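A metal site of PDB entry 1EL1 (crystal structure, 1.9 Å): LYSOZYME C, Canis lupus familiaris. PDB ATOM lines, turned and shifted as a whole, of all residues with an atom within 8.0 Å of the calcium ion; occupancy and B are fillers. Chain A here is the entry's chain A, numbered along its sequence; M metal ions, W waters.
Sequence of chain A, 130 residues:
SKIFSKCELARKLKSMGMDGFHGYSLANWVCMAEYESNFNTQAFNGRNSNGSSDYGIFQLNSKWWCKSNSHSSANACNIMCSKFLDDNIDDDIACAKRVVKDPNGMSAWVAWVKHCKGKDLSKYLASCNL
Water W2 lies within hydrogen-bond range of OD2 of Asp 91 (2.4 Å) and OD2 of Asp 86 (2.4 Å).
The calcium ion is bound by the backbone carbonyl oxygen of Asn 88, the backbone carbonyl oxygen of Lys 83, the side-chain carboxylate of Asp 86, the side-chain carboxylate of Asp 92, the side-chain carboxylate of Asp 91, water W1 and water W2.
ND2 of Asn 88 is in hydrogen-bond range of OD1 of Asp 90 (2.7 Å).
Of the 18 residues printed, 5 come within 4 Å of the calcium ion.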
ATOM      1  N   THR A  41      14.924  18.204  -9.300  1.00  0.00           N
ATOM      2  CA  THR A  41      14.238  17.610 -10.448  1.00  0.00           C
ATOM      3  C   THR A  41      14.165  16.088 -10.374  1.00  0.00           C
ATOM      4  O   THR A  41      13.330  15.472 -11.020  1.00  0.00           O
ATOM      5  CB  THR A  41      14.914  18.020 -11.787  1.00  0.00           C
ATOM      6  OG1 THR A  41      16.254  17.527 -11.822  1.00  0.00           O
ATOM      7  CG2 THR A  41      14.940  19.525 -11.927  1.00  0.00           C
ATOM      8  N   GLY A  56       9.474  13.932  -9.606  1.00  0.00           N
ATOM      9  CA  GLY A  56      10.014  15.237  -9.942  1.00  0.00           C
ATOM     10  C   GLY A  56       9.869  16.456  -9.065  1.00  0.00           C
ATOM     11  O   GLY A  56       9.362  16.415  -7.946  1.00  0.00           O
ATOM     12  N   ILE A  57      10.338  17.567  -9.630  1.00  0.00           N
ATOM     13  CA  ILE A  57      10.334  18.870  -8.985  1.00  0.00           C
ATOM     14  C   ILE A  57       8.998  19.283  -8.372  1.00  0.00           C
ATOM     15  O   ILE A  57       8.956  20.015  -7.384  1.00  0.00           O
ATOM     16  CB  ILE A  57      10.834  19.938 -10.012  1.00  0.00           C
ATOM     17  CG1 ILE A  57      11.259  21.218  -9.289  1.00  0.00           C
ATOM     18  CG2 ILE A  57       9.766  20.212 -11.042  1.00  0.00           C
ATOM     19  CD1 ILE A  57      11.971  22.203 -10.203  1.00  0.00           C
ATOM     20  N   ILE A  79       1.845  11.058 -20.332  1.00  0.00           N
ATOM     21  CA  ILE A  79       3.301  11.066 -20.396  1.00  0.00           C
ATOM     22  C   ILE A  79       3.776  10.067 -19.344  1.00  0.00           C
ATOM     23  O   ILE A  79       3.113   9.883 -18.323  1.00  0.00           O
ATOM     24  CB  ILE A  79       3.852  12.467 -20.040  1.00  0.00           C
ATOM     25  CG1 ILE A  79       5.384  12.471 -20.099  1.00  0.00           C
ATOM     26  CG2 ILE A  79       3.378  12.849 -18.643  1.00  0.00           C
ATOM     27  CD1 ILE A  79       6.010  13.780 -19.669  1.00  0.00           C
ATOM     28  N   MET A  80       4.911   9.429 -19.581  1.00  0.00           N
ATOM     29  CA  MET A  80       5.429   8.471 -18.614  1.00  0.00           C
ATOM     30  C   MET A  80       6.006   9.245 -17.424  1.00  0.00           C
ATOM     31  O   MET A  80       6.496  10.363 -17.580  1.00  0.00           O
ATOM     32  CB  MET A  80       6.499   7.571 -19.249  1.00  0.00           C
ATOM     33  CG  MET A  80       6.011   6.769 -20.478  1.00  0.00           C
ATOM     34  SD  MET A  80       4.457   5.822 -20.258  1.00  0.00           S
ATOM     35  CE  MET A  80       5.015   4.473 -19.170  1.00  0.00           C
ATOM     36  N   CYS A  81       5.937   8.646 -16.242  1.00  0.00           N
ATOM     37  CA  CYS A  81       6.431   9.282 -15.027  1.00  0.00           C
ATOM     38  C   CYS A  81       7.945   9.558 -15.033  1.00  0.00           C
ATOM     39  O   CYS A  81       8.406  10.523 -14.438  1.00  0.00           O
ATOM     40  CB  CYS A  81       6.095   8.422 -13.823  1.00  0.00           C
ATOM     41  SG  CYS A  81       4.320   8.155 -13.541  1.00  0.00           S
ATOM     42  N   SER A  82       8.700   8.672 -15.690  1.00  0.00           N
ATOM     43  CA  SER A  82      10.148   8.795 -15.789  1.00  0.00           C
ATOM     44  C   SER A  82      10.565  10.125 -16.405  1.00  0.00           C
ATOM     45  O   SER A  82      11.620  10.667 -16.089  1.00  0.00           O
ATOM     46  CB  SER A  82      10.727   7.645 -16.610  1.00  0.00           C
ATOM     47  OG  SER A  82      10.288   7.714 -17.961  1.00  0.00           O
ATOM     48  N   LYS A  83       9.727  10.648 -17.290  1.00  0.00           N
ATOM     49  CA  LYS A  83      10.022  11.919 -17.919  1.00  0.00           C
ATOM     50  C   LYS A  83      10.201  12.961 -16.836  1.00  0.00           C
ATOM     51  O   LYS A  83      10.510  14.276 -17.211  1.00  0.00           O
ATOM     52  CB  LYS A  83       8.885  12.342 -18.844  1.00  0.00           C
ATOM     53  CG  LYS A  83       8.714  11.465 -20.070  1.00  0.00           C
ATOM     54  CD  LYS A  83       9.985  11.475 -20.909  1.00  0.00           C
ATOM     55  CE  LYS A  83       9.840  10.604 -22.150  1.00  0.00           C
ATOM     56  NZ  LYS A  83      11.083  10.604 -22.966  1.00  0.00           N
ATOM     57  N   PHE A  84       9.429  12.844 -15.750  1.00  0.00           N
ATOM     58  CA  PHE A  84       9.492  13.791 -14.640  1.00  0.00           C
ATOM     59  C   PHE A  84      10.731  13.646 -13.779  1.00  0.00           C
ATOM     60  O   PHE A  84      10.860  14.324 -12.766  1.00  0.00           O
ATOM     61  CB  PHE A  84       8.266  13.662 -13.747  1.00  0.00           C
ATOM     62  CG  PHE A  84       6.978  13.880 -14.468  1.00  0.00           C
ATOM     63  CD1 PHE A  84       6.911  14.734 -15.564  1.00  0.00           C
ATOM     64  CD2 PHE A  84       5.808  13.272 -14.021  1.00  0.00           C
ATOM     65  CE1 PHE A  84       5.708  14.984 -16.215  1.00  0.00           C
ATOM     66  CE2 PHE A  84       4.596  13.501 -14.662  1.00  0.00           C
ATOM     67  CZ  PHE A  84       4.550  14.365 -15.760  1.00  0.00           C
ATOM     68  N   LEU A  85      11.630  12.748 -14.168  1.00  0.00           N
ATOM     69  CA  LEU A  85      12.851  12.535 -13.414  1.00  0.00           C
ATOM     70  C   LEU A  85      14.090  13.001 -14.180  1.00  0.00           C
ATOM     71  O   LEU A  85      15.205  12.912 -13.675  1.00  0.00           O
ATOM     72  CB  LEU A  85      12.975  11.060 -13.018  1.00  0.00           C
ATOM     73  CG  LEU A  85      11.904  10.535 -12.071  1.00  0.00           C
ATOM     74  CD1 LEU A  85      12.226   9.113 -11.682  1.00  0.00           C
ATOM     75  CD2 LEU A  85      11.817  11.397 -10.822  1.00  0.00           C
ATOM     76  N   ASP A  86      13.960  13.558 -15.269  1.00  0.00           N
ATOM     77  CA  ASP A  86      15.013  13.980 -16.181  1.00  0.00           C
ATOM     78  C   ASP A  86      15.265  15.478 -15.950  1.00  0.00           C
ATOM     79  O   ASP A  86      14.721  16.064 -15.016  1.00  0.00           O
ATOM     80  CB  ASP A  86      14.669  13.660 -17.648  1.00  0.00           C
ATOM     81  CG  ASP A  86      13.382  14.303 -18.098  1.00  0.00           C
ATOM     82  OD1 ASP A  86      13.043  15.368 -17.561  1.00  0.00           O
ATOM     83  OD2 ASP A  86      12.716  13.747 -19.004  1.00  0.00           O
ATOM     84  N   ASP A  87      16.141  16.147 -16.482  1.00  0.00           N
ATOM     85  CA  ASP A  87      16.524  17.507 -16.117  1.00  0.00           C
ATOM     86  C   ASP A  87      15.846  18.684 -16.818  1.00  0.00           C
ATOM     87  O   ASP A  87      16.120  19.836 -16.481  1.00  0.00           O
ATOM     88  CB  ASP A  87      18.033  17.628 -16.261  1.00  0.00           C
ATOM     89  CG  ASP A  87      18.780  16.609 -15.418  1.00  0.00           C
ATOM     90  OD1 ASP A  87      18.908  16.843 -14.195  1.00  0.00           O
ATOM     91  OD2 ASP A  87      19.227  15.574 -15.972  1.00  0.00           O
ATOM     92  N   ASN A  88      14.983  18.404 -17.781  1.00  0.00           N
ATOM     93  CA  ASN A  88      14.284  19.472 -18.495  1.00  0.00           C
ATOM     94  C   ASN A  88      12.881  19.518 -17.934  1.00  0.00           C
ATOM     95  O   ASN A  88      12.210  18.416 -17.778  1.00  0.00           O
ATOM     96  CB  ASN A  88      14.231  19.171 -19.987  1.00  0.00           C
ATOM     97  CG  ASN A  88      13.979  20.417 -20.815  1.00  0.00           C
ATOM     98  OD1 ASN A  88      14.909  21.035 -21.336  1.00  0.00           O
ATOM     99  ND2 ASN A  88      12.715  20.793 -20.924  1.00  0.00           N
ATOM    100  N   ILE A  89      12.566  20.533 -17.131  1.00  0.00           N
ATOM    101  CA  ILE A  89      11.237  20.583 -16.504  1.00  0.00           C
ATOM    102  C   ILE A  89      10.151  21.176 -17.423  1.00  0.00           C
ATOM    103  O   ILE A  89       9.113  21.622 -16.952  1.00  0.00           O
ATOM    104  CB  ILE A  89      11.289  21.391 -15.203  1.00  0.00           C
ATOM    105  CG1 ILE A  89      11.789  22.808 -15.458  1.00  0.00           C
ATOM    106  CG2 ILE A  89      12.174  20.674 -14.188  1.00  0.00           C
ATOM    107  CD1 ILE A  89      11.631  23.735 -14.273  1.00  0.00           C
ATOM    108  N   ASP A  90      10.381  21.148 -18.722  1.00  0.00           N
ATOM    109  CA  ASP A  90       9.430  21.730 -19.672  1.00  0.00           C
ATOM    110  C   ASP A  90       8.138  20.954 -19.716  1.00  0.00           C
ATOM    111  O   ASP A  90       7.067  21.503 -20.025  1.00  0.00           O
ATOM    112  CB  ASP A  90      10.047  21.806 -21.079  1.00  0.00           C
ATOM    113  CG  ASP A  90      10.980  22.995 -21.232  1.00  0.00           C
ATOM    114  OD1 ASP A  90      11.767  23.282 -20.306  1.00  0.00           O
ATOM    115  OD2 ASP A  90      10.926  23.647 -22.301  1.00  0.00           O
ATOM    116  N   ASP A  91       8.494  19.490 -19.534  1.00  0.00           N
ATOM    117  CA  ASP A  91       7.248  18.762 -19.532  1.00  0.00           C
ATOM    118  C   ASP A  91       6.688  18.574 -18.134  1.00  0.00           C
ATOM    119  O   ASP A  91       5.490  18.335 -18.000  1.00  0.00           O
ATOM    120  CB  ASP A  91       7.398  17.435 -20.223  1.00  0.00           C
ATOM    121  CG  ASP A  91       8.439  16.510 -19.619  1.00  0.00           C
ATOM    122  OD1 ASP A  91       8.405  16.341 -18.373  1.00  0.00           O
ATOM    123  OD2 ASP A  91       9.273  15.954 -20.377  1.00  0.00           O
ATOM    124  N   ASP A  92       7.160  18.888 -17.063  1.00  0.00           N
ATOM    125  CA  ASP A  92       6.627  18.823 -15.711  1.00  0.00           C
ATOM    126  C   ASP A  92       5.683  20.005 -15.499  1.00  0.00           C
ATOM    127  O   ASP A  92       4.652  19.877 -14.834  1.00  0.00           O
ATOM    128  CB  ASP A  92       7.733  18.873 -14.669  1.00  0.00           C
ATOM    129  CG  ASP A  92       8.849  17.902 -14.963  1.00  0.00           C
ATOM    130  OD1 ASP A  92       9.418  17.973 -16.063  1.00  0.00           O
ATOM    131  OD2 ASP A  92       9.145  17.072 -14.087  1.00  0.00           O
ATOM    132  N   ILE A  93       5.974  21.252 -16.072  1.00  0.00           N
ATOM    133  CA  ILE A  93       5.210  22.483 -15.964  1.00  0.00           C
ATOM    134  C   ILE A  93       3.872  22.306 -16.679  1.00  0.00           C
ATOM    135  O   ILE A  93       2.838  22.729 -16.172  1.00  0.00           O
ATOM    136  CB  ILE A  93       5.961  23.660 -16.624  1.00  0.00           C
ATOM    137  CG1 ILE A  93       7.217  23.977 -15.824  1.00  0.00           C
ATOM    138  CG2 ILE A  93       5.067  24.886 -16.698  1.00  0.00           C
ATOM    139  CD1 ILE A  93       8.087  25.057 -16.436  1.00  0.00           C
HETATM  140 CA    CA M   1      10.854  16.558 -17.593  1.00  0.00          CA
HETATM  141  O   HOH W   1      12.385  16.450 -15.363  1.00  0.00           O
HETATM  142  O   HOH W   2      11.671  15.697 -20.054  1.00  0.00           O
